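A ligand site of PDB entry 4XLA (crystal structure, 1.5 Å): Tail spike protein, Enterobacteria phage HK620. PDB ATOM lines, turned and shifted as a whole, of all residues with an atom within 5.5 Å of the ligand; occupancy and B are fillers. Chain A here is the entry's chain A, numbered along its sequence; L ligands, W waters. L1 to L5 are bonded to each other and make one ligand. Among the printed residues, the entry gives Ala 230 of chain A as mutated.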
ATOM      1  N   GLY A 102     -16.966 -22.599  -7.017  1.00  0.00           N
ATOM      2  CA  GLY A 102     -17.082 -21.318  -6.301  1.00  0.00           C
ATOM      3  C   GLY A 102     -16.904 -21.509  -4.797  1.00  0.00           C
ATOM      4  O   GLY A 102     -16.729 -20.498  -4.086  1.00  0.00           O
ATOM      5  N   HIS A 103     -16.851 -22.746  -4.287  1.00  0.00           N
ATOM      6  CA  HIS A 103     -16.746 -23.043  -2.873  1.00  0.00           C
ATOM      7  C   HIS A 103     -15.427 -23.707  -2.615  1.00  0.00           C
ATOM      8  O   HIS A 103     -15.235 -24.319  -1.592  1.00  0.00           O
ATOM      9  CB  HIS A 103     -17.899 -23.970  -2.435  1.00  0.00           C
ATOM     10  CG  HIS A 103     -19.259 -23.456  -2.741  1.00  0.00           C
ATOM     11  ND1 HIS A 103     -19.948 -22.639  -1.876  1.00  0.00           N
ATOM     12  CD2 HIS A 103     -20.057 -23.585  -3.819  1.00  0.00           C
ATOM     13  CE1 HIS A 103     -21.106 -22.318  -2.397  1.00  0.00           C
ATOM     14  NE2 HIS A 103     -21.199 -22.876  -3.581  1.00  0.00           N
ATOM     15  N   SER A 104     -14.484 -23.651  -3.597  1.00  0.00           N
ATOM     16  CA  SER A 104     -13.193 -24.384  -3.472  1.00  0.00           C
ATOM     17  C   SER A 104     -13.468 -25.845  -3.199  1.00  0.00           C
ATOM     18  O   SER A 104     -12.694 -26.529  -2.551  1.00  0.00           O
ATOM     19  CB  SER A 104     -12.317 -23.789  -2.389  1.00  0.00           C
ATOM     20  OG  SER A 104     -12.198 -22.407  -2.675  1.00  0.00           O
ATOM     21  N   GLN A 133     -12.923 -27.038   0.341  1.00  0.00           N
ATOM     22  CA  GLN A 133     -14.039 -27.633   1.083  1.00  0.00           C
ATOM     23  C   GLN A 133     -14.216 -28.976   0.552  1.00  0.00           C
ATOM     24  O   GLN A 133     -14.534 -29.138  -0.658  1.00  0.00           O
ATOM     25  CB  GLN A 133     -15.277 -26.777   0.926  1.00  0.00           C
ATOM     26  CG  GLN A 133     -15.068 -25.368   1.516  1.00  0.00           C
ATOM     27  CD  GLN A 133     -16.370 -24.613   1.680  1.00  0.00           C
ATOM     28  OE1 GLN A 133     -17.281 -25.004   2.428  1.00  0.00           O
ATOM     29  NE2 GLN A 133     -16.479 -23.455   1.052  1.00  0.00           N
ATOM     30  N   PHE A 138     -23.752 -27.798  -2.106  1.00  0.00           N
ATOM     31  CA  PHE A 138     -24.320 -26.789  -3.050  1.00  0.00           C
ATOM     32  C   PHE A 138     -24.126 -27.318  -4.460  1.00  0.00           C
ATOM     33  O   PHE A 138     -23.186 -28.024  -4.735  1.00  0.00           O
ATOM     34  CB  PHE A 138     -23.602 -25.473  -2.899  1.00  0.00           C
ATOM     35  CG  PHE A 138     -23.781 -24.787  -1.516  1.00  0.00           C
ATOM     36  CD1 PHE A 138     -24.982 -24.192  -1.166  1.00  0.00           C
ATOM     37  CD2 PHE A 138     -22.726 -24.718  -0.641  1.00  0.00           C
ATOM     38  CE1 PHE A 138     -25.085 -23.526   0.096  1.00  0.00           C
ATOM     39  CE2 PHE A 138     -22.798 -24.054   0.565  1.00  0.00           C
ATOM     40  CZ  PHE A 138     -23.988 -23.472   0.929  1.00  0.00           C
ATOM     41  N   PRO A 143     -24.711 -19.527  -3.400  1.00  0.00           N
ATOM     42  CA  PRO A 143     -25.619 -20.360  -2.605  1.00  0.00           C
ATOM     43  C   PRO A 143     -27.088 -19.973  -2.747  1.00  0.00           C
ATOM     44  O   PRO A 143     -28.013 -20.810  -2.661  1.00  0.00           O
ATOM     45  CB  PRO A 143     -25.093 -20.165  -1.191  1.00  0.00           C
ATOM     46  CG  PRO A 143     -24.197 -19.009  -1.209  1.00  0.00           C
ATOM     47  CD  PRO A 143     -23.619 -18.984  -2.613  1.00  0.00           C
ATOM     48  N   LEU A 173     -10.689 -19.939   3.307  1.00  0.00           N
ATOM     49  CA  LEU A 173     -11.693 -20.792   4.057  1.00  0.00           C
ATOM     50  C   LEU A 173     -11.374 -22.247   3.767  1.00  0.00           C
ATOM     51  O   LEU A 173     -11.020 -22.619   2.633  1.00  0.00           O
ATOM     52  CB  LEU A 173     -13.154 -20.551   3.579  1.00  0.00           C
ATOM     53  CG  LEU A 173     -13.615 -19.147   3.899  1.00  0.00           C
ATOM     54  CD1 LEU A 173     -14.894 -18.767   3.163  1.00  0.00           C
ATOM     55  CD2 LEU A 173     -13.669 -18.789   5.360  1.00  0.00           C
ATOM     56  N   ASN A 175     -13.030 -26.255   4.885  1.00  0.00           N
ATOM     57  CA  ASN A 175     -14.179 -26.987   5.468  1.00  0.00           C
ATOM     58  C   ASN A 175     -13.957 -28.480   5.121  1.00  0.00           C
ATOM     59  O   ASN A 175     -13.444 -28.833   4.073  1.00  0.00           O
ATOM     60  CB  ASN A 175     -15.501 -26.487   4.898  1.00  0.00           C
ATOM     61  CG  ASN A 175     -16.730 -26.871   5.721  1.00  0.00           C
ATOM     62  OD1 ASN A 175     -16.690 -27.498   6.796  1.00  0.00           O
ATOM     63  ND2 ASN A 175     -17.866 -26.431   5.215  1.00  0.00           N
ATOM     64  N   THR A 198     -11.216 -23.918   8.812  1.00  0.00           N
ATOM     65  CA  THR A 198     -12.148 -22.975   9.407  1.00  0.00           C
ATOM     66  C   THR A 198     -13.248 -23.731  10.162  1.00  0.00           C
ATOM     67  O   THR A 198     -13.592 -23.374  11.310  1.00  0.00           O
ATOM     68  CB  THR A 198     -12.801 -22.126   8.311  1.00  0.00           C
ATOM     69  OG1 THR A 198     -11.783 -21.551   7.446  1.00  0.00           O
ATOM     70  CG2 THR A 198     -13.645 -21.057   8.880  1.00  0.00           C
ATOM     71  N   TRP A 199     -13.843 -24.692   9.455  1.00  0.00           N
ATOM     72  CA  TRP A 199     -14.875 -25.600  10.022  1.00  0.00           C
ATOM     73  C   TRP A 199     -14.535 -27.061   9.627  1.00  0.00           C
ATOM     74  O   TRP A 199     -13.813 -27.261   8.625  1.00  0.00           O
ATOM     75  CB  TRP A 199     -16.237 -25.300   9.444  1.00  0.00           C
ATOM     76  CG  TRP A 199     -16.670 -23.835   9.493  1.00  0.00           C
ATOM     77  CD1 TRP A 199     -17.040 -23.114  10.571  1.00  0.00           C
ATOM     78  CD2 TRP A 199     -16.694 -22.935   8.375  1.00  0.00           C
ATOM     79  NE1 TRP A 199     -17.407 -21.845  10.208  1.00  0.00           N
ATOM     80  CE2 TRP A 199     -17.108 -21.668   8.865  1.00  0.00           C
ATOM     81  CE3 TRP A 199     -16.369 -23.078   7.031  1.00  0.00           C
ATOM     82  CZ2 TRP A 199     -17.298 -20.582   8.003  1.00  0.00           C
ATOM     83  CZ3 TRP A 199     -16.495 -21.987   6.192  1.00  0.00           C
ATOM     84  CH2 TRP A 199     -16.929 -20.761   6.683  1.00  0.00           C
ATOM     85  N   THR A 202     -20.296 -27.878   8.166  1.00  0.00           N
ATOM     86  CA  THR A 202     -21.341 -26.903   8.220  1.00  0.00           C
ATOM     87  C   THR A 202     -22.673 -27.470   7.730  1.00  0.00           C
ATOM     88  O   THR A 202     -22.696 -28.316   6.811  1.00  0.00           O
ATOM     89  CB  THR A 202     -21.053 -25.659   7.398  1.00  0.00           C
ATOM     90  OG1 THR A 202     -20.949 -25.961   5.982  1.00  0.00           O
ATOM     91  CG2 THR A 202     -19.700 -25.073   7.826  1.00  0.00           C
ATOM     92  N   LEU A 203     -23.737 -27.087   8.420  1.00  0.00           N
ATOM     93  CA  LEU A 203     -25.085 -27.577   8.163  1.00  0.00           C
ATOM     94  C   LEU A 203     -25.938 -26.448   7.704  1.00  0.00           C
ATOM     95  O   LEU A 203     -25.980 -25.411   8.421  1.00  0.00           O
ATOM     96  CB  LEU A 203     -25.722 -28.209   9.419  1.00  0.00           C
ATOM     97  CG  LEU A 203     -24.849 -29.233  10.136  1.00  0.00           C
ATOM     98  CD1 LEU A 203     -25.648 -29.702  11.369  1.00  0.00           C
ATOM     99  CD2 LEU A 203     -24.477 -30.359   9.218  1.00  0.00           C
ATOM    100  N   GLY A 204     -26.666 -26.562   6.605  1.00  0.00           N
ATOM    101  CA  GLY A 204     -27.542 -25.495   6.201  1.00  0.00           C
ATOM    102  C   GLY A 204     -26.852 -24.349   5.512  1.00  0.00           C
ATOM    103  O   GLY A 204     -25.603 -24.240   5.487  1.00  0.00           O
ATOM    104  N   TRP A 205     -27.662 -23.383   5.125  1.00  0.00           N
ATOM    105  CA  TRP A 205     -27.160 -22.139   4.534  1.00  0.00           C
ATOM    106  C   TRP A 205     -28.129 -21.065   4.812  1.00  0.00           C
ATOM    107  O   TRP A 205     -29.283 -21.098   4.297  1.00  0.00           O
ATOM    108  CB  TRP A 205     -26.862 -22.198   3.027  1.00  0.00           C
ATOM    109  CG  TRP A 205     -26.431 -20.883   2.505  1.00  0.00           C
ATOM    110  CD1 TRP A 205     -25.268 -20.284   2.737  1.00  0.00           C
ATOM    111  CD2 TRP A 205     -27.266 -19.936   1.832  1.00  0.00           C
ATOM    112  NE1 TRP A 205     -25.264 -19.010   2.199  1.00  0.00           N
ATOM    113  CE2 TRP A 205     -26.476 -18.783   1.610  1.00  0.00           C
ATOM    114  CE3 TRP A 205     -28.553 -19.989   1.314  1.00  0.00           C
ATOM    115  CZ2 TRP A 205     -26.978 -17.675   0.928  1.00  0.00           C
ATOM    116  CZ3 TRP A 205     -29.055 -18.916   0.646  1.00  0.00           C
ATOM    117  CH2 TRP A 205     -28.254 -17.753   0.457  1.00  0.00           C
ATOM    118  N   ASN A 206     -27.762 -20.129   5.690  1.00  0.00           N
ATOM    119  CA  ASN A 206     -28.644 -18.972   6.014  1.00  0.00           C
ATOM    120  C   ASN A 206     -30.054 -19.320   6.328  1.00  0.00           C
ATOM    121  O   ASN A 206     -30.997 -18.693   5.878  1.00  0.00           O
ATOM    122  CB  ASN A 206     -28.489 -17.812   5.033  1.00  0.00           C
ATOM    123  CG  ASN A 206     -27.116 -17.251   5.009  1.00  0.00           C
ATOM    124  OD1 ASN A 206     -26.233 -17.627   5.779  1.00  0.00           O
ATOM    125  ND2 ASN A 206     -26.875 -16.331   4.054  1.00  0.00           N
ATOM    126  N   ALA A 230      -9.732 -18.183  12.353  1.00  0.00           N
ATOM    127  CA  ALA A 230     -10.800 -18.553  13.254  1.00  0.00           C
ATOM    128  C   ALA A 230     -11.214 -19.956  12.946  1.00  0.00           C
ATOM    129  O   ALA A 230     -11.195 -20.414  11.800  1.00  0.00           O
ATOM    130  CB  ALA A 230     -12.003 -17.652  13.031  1.00  0.00           C
ATOM    131  N   HIS A 231     -11.677 -20.657  13.962  1.00  0.00           N
ATOM    132  CA  HIS A 231     -12.156 -22.012  13.717  1.00  0.00           C
ATOM    133  C   HIS A 231     -13.369 -22.314  14.557  1.00  0.00           C
ATOM    134  O   HIS A 231     -13.341 -22.095  15.771  1.00  0.00           O
ATOM    135  CB  HIS A 231     -11.080 -22.993  14.088  1.00  0.00           C
ATOM    136  CG  HIS A 231     -11.541 -24.406  14.060  1.00  0.00           C
ATOM    137  ND1 HIS A 231     -11.324 -25.252  12.991  1.00  0.00           N
ATOM    138  CD2 HIS A 231     -12.210 -25.144  14.992  1.00  0.00           C
ATOM    139  CE1 HIS A 231     -11.887 -26.414  13.247  1.00  0.00           C
ATOM    140  NE2 HIS A 231     -12.423 -26.366  14.449  1.00  0.00           N
ATOM    141  N   SER A 232     -14.428 -22.843  13.934  1.00  0.00           N
ATOM    142  CA  SER A 232     -15.550 -23.445  14.680  1.00  0.00           C
ATOM    143  C   SER A 232     -15.900 -24.810  14.087  1.00  0.00           C
ATOM    144  O   SER A 232     -16.079 -24.949  12.892  1.00  0.00           O
ATOM    145  CB  SER A 232     -16.766 -22.552  14.642  1.00  0.00           C
ATOM    146  OG  SER A 232     -16.463 -21.364  15.425  1.00  0.00           O
ATOM    147  N   TYR A 235     -20.715 -25.674  12.395  1.00  0.00           N
ATOM    148  CA  TYR A 235     -21.547 -24.457  12.285  1.00  0.00           C
ATOM    149  C   TYR A 235     -22.946 -24.872  11.817  1.00  0.00           C
ATOM    150  O   TYR A 235     -23.109 -25.396  10.692  1.00  0.00           O
ATOM    151  CB  TYR A 235     -20.865 -23.492  11.322  1.00  0.00           C
ATOM    152  CG  TYR A 235     -21.300 -22.043  11.318  1.00  0.00           C
ATOM    153  CD1 TYR A 235     -22.478 -21.633  10.774  1.00  0.00           C
ATOM    154  CD2 TYR A 235     -20.465 -21.039  11.828  1.00  0.00           C
ATOM    155  CE1 TYR A 235     -22.834 -20.287  10.727  1.00  0.00           C
ATOM    156  CE2 TYR A 235     -20.814 -19.718  11.750  1.00  0.00           C
ATOM    157  CZ  TYR A 235     -21.979 -19.339  11.221  1.00  0.00           C
ATOM    158  OH  TYR A 235     -22.307 -18.013  11.132  1.00  0.00           O
ATOM    159  N   ASN A 237     -26.407 -23.994  10.684  1.00  0.00           N
ATOM    160  CA  ASN A 237     -27.035 -22.853  10.050  1.00  0.00           C
ATOM    161  C   ASN A 237     -28.357 -23.237   9.331  1.00  0.00           C
ATOM    162  O   ASN A 237     -28.791 -22.636   8.388  1.00  0.00           O
ATOM    163  CB  ASN A 237     -26.056 -22.158   9.070  1.00  0.00           C
ATOM    164  CG  ASN A 237     -26.413 -20.686   8.873  1.00  0.00           C
ATOM    165  OD1 ASN A 237     -27.258 -20.121   9.550  1.00  0.00           O
ATOM    166  ND2 ASN A 237     -25.701 -20.039   7.944  1.00  0.00           N
ATOM    167  N   CYS A 260     -13.591 -22.701  18.540  1.00  0.00           N
ATOM    168  CA  CYS A 260     -14.879 -22.947  19.151  1.00  0.00           C
ATOM    169  C   CYS A 260     -15.410 -24.316  18.687  1.00  0.00           C
ATOM    170  O   CYS A 260     -15.166 -24.700  17.497  1.00  0.00           O
ATOM    171  CB  CYS A 260     -15.850 -21.858  18.773  1.00  0.00           C
ATOM    172  SG  CYS A 260     -17.423 -21.978  19.683  1.00  0.00           S
ATOM    173  N   GLU A 263     -21.294 -23.847  16.700  1.00  0.00           N
ATOM    174  CA  GLU A 263     -22.078 -22.623  16.621  1.00  0.00           C
ATOM    175  C   GLU A 263     -23.497 -22.972  16.238  1.00  0.00           C
ATOM    176  O   GLU A 263     -23.739 -23.682  15.265  1.00  0.00           O
ATOM    177  CB  GLU A 263     -21.525 -21.530  15.721  1.00  0.00           C
ATOM    178  CG  GLU A 263     -20.041 -21.244  15.988  1.00  0.00           C
ATOM    179  CD  GLU A 263     -19.598 -19.857  15.607  1.00  0.00           C
ATOM    180  OE1 GLU A 263     -20.438 -19.015  15.258  1.00  0.00           O
ATOM    181  OE2 GLU A 263     -18.364 -19.605  15.636  1.00  0.00           O
ATOM    182  N   HIS A 265     -26.927 -21.329  15.047  1.00  0.00           N
ATOM    183  CA  HIS A 265     -27.265 -20.087  14.364  1.00  0.00           C
ATOM    184  C   HIS A 265     -28.702 -20.002  13.871  1.00  0.00           C
ATOM    185  O   HIS A 265     -29.067 -19.023  13.257  1.00  0.00           O
ATOM    186  CB  HIS A 265     -26.285 -19.843  13.218  1.00  0.00           C
ATOM    187  CG  HIS A 265     -25.012 -19.228  13.657  1.00  0.00           C
ATOM    188  ND1 HIS A 265     -24.882 -17.878  13.913  1.00  0.00           N
ATOM    189  CD2 HIS A 265     -23.811 -19.756  13.859  1.00  0.00           C
ATOM    190  CE1 HIS A 265     -23.668 -17.617  14.317  1.00  0.00           C
ATOM    191  NE2 HIS A 265     -23.005 -18.754  14.351  1.00  0.00           N
ATOM    192  N   TYR A 284     -21.022 -20.814  20.305  1.00  0.00           N
ATOM    193  CA  TYR A 284     -21.802 -19.630  20.040  1.00  0.00           C
ATOM    194  C   TYR A 284     -23.286 -19.988  19.842  1.00  0.00           C
ATOM    195  O   TYR A 284     -23.614 -20.982  19.211  1.00  0.00           O
ATOM    196  CB  TYR A 284     -21.322 -18.923  18.791  1.00  0.00           C
ATOM    197  CG  TYR A 284     -20.015 -18.176  18.942  1.00  0.00           C
ATOM    198  CD1 TYR A 284     -18.781 -18.803  18.804  1.00  0.00           C
ATOM    199  CD2 TYR A 284     -20.031 -16.856  19.355  1.00  0.00           C
ATOM    200  CE1 TYR A 284     -17.596 -18.076  18.993  1.00  0.00           C
ATOM    201  CE2 TYR A 284     -18.840 -16.118  19.524  1.00  0.00           C
ATOM    202  CZ  TYR A 284     -17.655 -16.756  19.396  1.00  0.00           C
ATOM    203  OH  TYR A 284     -16.462 -16.028  19.573  1.00  0.00           O
ATOM    204  N   VAL A 286     -26.181 -17.655  18.471  1.00  0.00           N
ATOM    205  CA  VAL A 286     -26.242 -16.281  17.892  1.00  0.00           C
ATOM    206  C   VAL A 286     -27.331 -16.290  16.807  1.00  0.00           C
ATOM    207  O   VAL A 286     -27.346 -17.177  15.947  1.00  0.00           O
ATOM    208  CB  VAL A 286     -24.867 -15.922  17.330  1.00  0.00           C
ATOM    209  CG1 VAL A 286     -24.885 -14.599  16.555  1.00  0.00           C
ATOM    210  CG2 VAL A 286     -23.873 -15.763  18.418  1.00  0.00           C
ATOM    211  N   HIS A 288     -27.814 -14.077  13.713  1.00  0.00           N
ATOM    212  CA  HIS A 288     -27.278 -13.040  12.839  1.00  0.00           C
ATOM    213  C   HIS A 288     -28.390 -12.607  11.868  1.00  0.00           C
ATOM    214  O   HIS A 288     -28.925 -13.448  11.135  1.00  0.00           O
ATOM    215  CB  HIS A 288     -26.186 -13.595  11.968  1.00  0.00           C
ATOM    216  CG  HIS A 288     -24.867 -13.729  12.599  1.00  0.00           C
ATOM    217  ND1 HIS A 288     -24.318 -12.778  13.418  1.00  0.00           N
ATOM    218  CD2 HIS A 288     -23.967 -14.743  12.568  1.00  0.00           C
ATOM    219  CE1 HIS A 288     -23.115 -13.169  13.811  1.00  0.00           C
ATOM    220  NE2 HIS A 288     -22.880 -14.354  13.305  1.00  0.00           N
ATOM    221  N   ALA A 290     -27.906 -11.212   9.224  1.00  0.00           N
ATOM    222  CA  ALA A 290     -27.408 -11.564   7.888  1.00  0.00           C
ATOM    223  C   ALA A 290     -27.728 -13.000   7.461  1.00  0.00           C
ATOM    224  O   ALA A 290     -27.525 -13.364   6.272  1.00  0.00           O
ATOM    225  CB  ALA A 290     -25.900 -11.338   7.796  1.00  0.00           C
ATOM    226  N   GLU A 291     -28.092 -13.860   8.418  1.00  0.00           N
ATOM    227  CA  GLU A 291     -28.374 -15.275   8.176  1.00  0.00           C
ATOM    228  C   GLU A 291     -29.803 -15.652   8.289  1.00  0.00           C
ATOM    229  O   GLU A 291     -30.164 -16.829   8.321  1.00  0.00           O
ATOM    230  CB  GLU A 291     -27.548 -16.181   9.125  1.00  0.00           C
ATOM    231  CG  GLU A 291     -26.041 -16.014   8.884  1.00  0.00           C
ATOM    232  CD  GLU A 291     -25.164 -16.846   9.788  1.00  0.00           C
ATOM    233  OE1 GLU A 291     -25.634 -17.199  10.879  1.00  0.00           O
ATOM    234  OE2 GLU A 291     -24.059 -17.183   9.381  1.00  0.00           O
ATOM    235  N   ASN A 362     -20.167  -8.607  15.606  1.00  0.00           N
ATOM    236  CA  ASN A 362     -18.885  -8.787  14.964  1.00  0.00           C
ATOM    237  C   ASN A 362     -18.136  -7.490  14.737  1.00  0.00           C
ATOM    238  O   ASN A 362     -16.923  -7.540  14.583  1.00  0.00           O
ATOM    239  CB  ASN A 362     -19.047  -9.574  13.631  1.00  0.00           C
ATOM    240  CG  ASN A 362     -19.312 -11.070  13.882  1.00  0.00           C
ATOM    241  OD1 ASN A 362     -19.154 -11.564  15.011  1.00  0.00           O
ATOM    242  ND2 ASN A 362     -19.679 -11.766  12.856  1.00  0.00           N
HETATM  243  C1  LIG L   1     -17.398 -16.728  14.966  1.00  0.00           C
HETATM  244  C2  LIG L   1     -17.786 -17.229  13.564  1.00  0.00           C
HETATM  245  C3  LIG L   1     -18.416 -16.055  12.813  1.00  0.00           C
HETATM  246  C4  LIG L   1     -19.600 -15.655  13.630  1.00  0.00           C
HETATM  247  C5  LIG L   1     -19.286 -15.326  15.147  1.00  0.00           C
HETATM  248  C6  LIG L   1     -20.534 -15.237  15.996  1.00  0.00           C
HETATM  249  C7  LIG L   1     -16.519 -18.977  12.282  1.00  0.00           C
HETATM  250  C8  LIG L   1     -15.205 -19.398  11.733  1.00  0.00           C
HETATM  251  N1  LIG L   1     -16.619 -17.745  12.912  1.00  0.00           N
HETATM  252  O1  LIG L   1     -16.796 -17.749  15.719  1.00  0.00           O
HETATM  253  O2  LIG L   1     -18.695 -16.392  11.503  1.00  0.00           O
HETATM  254  O3  LIG L   1     -20.270 -14.533  13.051  1.00  0.00           O
HETATM  255  O4  LIG L   1     -18.524 -16.339  15.701  1.00  0.00           O
HETATM  256  O5  LIG L   1     -21.323 -16.436  15.970  1.00  0.00           O
HETATM  257  O6  LIG L   1     -17.506 -19.728  12.184  1.00  0.00           O
HETATM  258  C1  LG2 L   2     -18.571 -15.316  10.529  1.00  0.00           C
HETATM  259  C2  LG2 L   2     -19.527 -15.619   9.369  1.00  0.00           C
HETATM  260  C3  LG2 L   2     -19.037 -16.908   8.630  1.00  0.00           C
HETATM  261  C4  LG2 L   2     -17.569 -16.923   8.290  1.00  0.00           C
HETATM  262  C5  LG2 L   2     -16.778 -16.587   9.541  1.00  0.00           C
HETATM  263  C6  LG2 L   2     -15.268 -16.520   9.301  1.00  0.00           C
HETATM  264  O1  LG2 L   2     -20.831 -15.725   9.906  1.00  0.00           O
HETATM  265  O2  LG2 L   2     -19.905 -16.950   7.507  1.00  0.00           O
HETATM  266  O3  LG2 L   2     -17.341 -15.853   7.306  1.00  0.00           O
HETATM  267  O4  LG2 L   2     -17.226 -15.390  10.180  1.00  0.00           O
HETATM  268  O5  LG2 L   2     -14.859 -17.724   8.595  1.00  0.00           O
HETATM  269  C1  LG3 L   3     -16.546 -16.338   6.208  1.00  0.00           C
HETATM  270  C2  LG3 L   3     -16.093 -15.069   5.444  1.00  0.00           C
HETATM  271  C3  LG3 L   3     -17.234 -14.362   4.757  1.00  0.00           C
HETATM  272  C4  LG3 L   3     -17.953 -15.346   3.884  1.00  0.00           C
HETATM  273  C5  LG3 L   3     -18.491 -16.501   4.772  1.00  0.00           C
HETATM  274  C6  LG3 L   3     -19.270 -17.567   4.039  1.00  0.00           C
HETATM  275  O1  LG3 L   3     -15.348 -14.184   6.283  1.00  0.00           O
HETATM  276  O2  LG3 L   3     -16.618 -13.332   3.933  1.00  0.00           O
HETATM  277  O3  LG3 L   3     -19.012 -14.696   3.286  1.00  0.00           O
HETATM  278  O4  LG3 L   3     -17.343 -17.120   5.329  1.00  0.00           O
HETATM  279  O5  LG3 L   3     -18.445 -18.091   2.966  1.00  0.00           O
HETATM  280  C1  LG4 L   4     -20.973 -17.947   7.580  1.00  0.00           C
HETATM  281  C2  LG4 L   4     -22.038 -17.548   6.545  1.00  0.00           C
HETATM  282  C3  LG4 L   4     -23.027 -18.707   6.402  1.00  0.00           C
HETATM  283  C4  LG4 L   4     -22.393 -20.091   6.312  1.00  0.00           C
HETATM  284  C5  LG4 L   4     -21.456 -20.251   7.455  1.00  0.00           C
HETATM  285  C6  LG4 L   4     -20.743 -21.557   7.464  1.00  0.00           C
HETATM  286  C7  LG4 L   4     -22.682 -15.202   6.297  1.00  0.00           C
HETATM  287  C8  LG4 L   4     -23.414 -14.033   6.904  1.00  0.00           C
HETATM  288  N1  LG4 L   4     -22.712 -16.336   6.965  1.00  0.00           N
HETATM  289  O1  LG4 L   4     -23.781 -18.453   5.217  1.00  0.00           O
HETATM  290  O2  LG4 L   4     -23.486 -21.033   6.492  1.00  0.00           O
HETATM  291  O3  LG4 L   4     -20.416 -19.256   7.363  1.00  0.00           O
HETATM  292  O4  LG4 L   4     -19.980 -21.740   6.279  1.00  0.00           O
HETATM  293  O5  LG4 L   4     -22.089 -15.067   5.249  1.00  0.00           O
HETATM  294  C1  LG5 L   5     -19.055 -17.874   1.701  1.00  0.00           C
HETATM  295  C2  LG5 L   5     -18.028 -18.337   0.653  1.00  0.00           C
HETATM  296  C3  LG5 L   5     -17.992 -19.829   0.533  1.00  0.00           C
HETATM  297  C4  LG5 L   5     -19.334 -20.451   0.496  1.00  0.00           C
HETATM  298  C5  LG5 L   5     -20.188 -19.975   1.665  1.00  0.00           C
HETATM  299  C6  LG5 L   5     -21.589 -20.559   1.610  1.00  0.00           C
HETATM  300  O1  LG5 L   5     -18.534 -17.886  -0.601  1.00  0.00           O
HETATM  301  O2  LG5 L   5     -17.209 -20.182  -0.671  1.00  0.00           O
HETATM  302  O3  LG5 L   5     -19.032 -21.849   0.571  1.00  0.00           O
HETATM  303  O4  LG5 L   5     -20.320 -18.531   1.593  1.00  0.00           O
HETATM  304  O   HOH W   1     -20.920 -23.709   4.601  1.00  0.00           O
HETATM  305  O   HOH W   2     -16.485 -13.146   8.572  1.00  0.00           O
HETATM  306  O   HOH W   3     -21.338 -17.430  -1.020  1.00  0.00           O
HETATM  307  O   HOH W   4     -12.646 -14.703   5.503  1.00  0.00           O
HETATM  308  O   HOH W   5     -20.541 -13.099   4.572  1.00  0.00           O
HETATM  309  O   HOH W   6     -16.148 -18.572  -2.305  1.00  0.00           O
HETATM  310  O   HOH W   7     -21.433 -12.999  10.222  1.00  0.00           O
HETATM  311  O   HOH W   8     -24.425 -14.795   3.422  1.00  0.00           O
HETATM  312  O   HOH W   9     -14.540 -15.504  12.868  1.00  0.00           O
HETATM  313  O   HOH W  10     -17.115 -14.040  17.193  1.00  0.00           O
HETATM  314  O   HOH W  11     -14.532 -19.330  15.546  1.00  0.00           O
HETATM  315  O   HOH W  12     -19.715 -23.891   2.242  1.00  0.00           O
HETATM  316  O   HOH W  13     -23.613 -22.695   4.393  1.00  0.00           O
HETATM  317  O   HOH W  14     -12.203 -17.480   8.911  1.00  0.00           O
HETATM  318  O   HOH W  15     -22.835 -17.277   2.555  1.00  0.00           O
HETATM  319  O   HOH W  16     -14.911 -16.506  17.243  1.00  0.00           O
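OE2 of Glu 263 is in hydrogen-bond range of O1 of LIG L1 (2.4 Å). A ring nitrogen (ND1) of His 103 lies within hydrogen-bond range of an oxygen (O3) of LG5 L5, 2.7 Å away. OE2 of Glu 291 is in hydrogen-bond range of N1 of LG4 L4 (2.9 Å). ND2 of Asn 237 lies within hydrogen-bond range of O2 of LG4 L4 (2.8 Å). A ring nitrogen (NE2) of His 288 is in hydrogen-bond range of an oxygen (O3) of LIG L1 (2.6 Å). The side-chain amide oxygen (OD1) of Asn 206 sits at hydrogen-bond distance from an oxygen (O1) of LG4 L4 (2.6 Å). The side-chain amide nitrogen of Gln 133 lies within hydrogen-bond range of an oxygen (O3) of LG5 L5, 3.1 Å away. O6 of LIG L1 sits at hydrogen-bond distance from NE1 of Trp 199, 2.9 Å away. OH of Tyr 235 lies within hydrogen-bond range of O1 of LG2 L2 (3.0 Å). An oxygen (O2) of LG5 L5 lies within hydrogen-bond range of the backbone carbonyl oxygen of Gly 102 (3.5 Å). The indole nitrogen (NE1) of Trp 205 sits at hydrogen-bond distance from an oxygen (O1) of LG4 L4, at 3.4 Å. ND2 of Asn 362 lies within hydrogen-bond range of O3 of LIG L1 (2.8 Å). A ring nitrogen (NE2) of His 265 sits close to an oxygen (O5) of LIG L1 (3.3 Å).
ND2 of Asn 237 lies close to N of Asn 206 (3.1 Å). O of His 103 is in hydrogen-bond range of NE2 of Gln 133 (3.0 Å). The side-chain amide oxygen (OE1) of Gln 133 sits at hydrogen-bond distance from the side-chain amide nitrogen (ND2) of Asn 175 (3.2 Å). The side-chain carboxylate (OE1) of Glu 263 is in hydrogen-bond range of a ring nitrogen (NE2) of His 265 (2.7 Å). O of Thr 198 lies within hydrogen-bond range of N of Ser 232. O of Leu 203 lies within hydrogen-bond range of N of Asn 237. OD1 of Asn 175 lies close to O of Trp 199, at 3.4 Å. ND2 of Asn 175 lies within hydrogen-bond range of OG1 of Thr 202 (3.2 Å).
Merely in contact with the ligand: Phe 138, Leu 173, Thr 198, Thr 202, Gly 204, Ala 230, Ser 232, Tyr 284, Val 286 and Ala 290. Hydrophobic or aromatic side chains within 4 Å of the ligand: His 103, Phe 138, Leu 173, Trp 199, Trp 205, Ala 230, Tyr 235, His 265, Tyr 284, Val 286, His 288 and Ala 290. Of the 29 residues printed, 23 come within 4 Å of the ligand.
Water W6 bridges O2 of LG5 L5 and O of Gly 102. Water W13 bridges O2 of LG4 L4 (2.7 Å) and O of Gly 204 (2.7 Å). Water W12 bridges OE1 of Gln 133 and O3 of LG5 L5. Water W11 lies within hydrogen-bond range of an oxygen (O1) of LIG L1 (2.8 Å), the side-chain hydroxyl (OG) of Ser 232 (2.8 Å) and the backbone carbonyl oxygen (O) of His 231 (3.0 Å). Water W8 bridges ND2 of Asn 206 (3.0 Å) and O5 of LG4 L4 (3.0 Å). Water W10 lies within hydrogen-bond range of O4 of LIG L1 (3.1 Å) and OH of Tyr 284 (3.2 Å).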
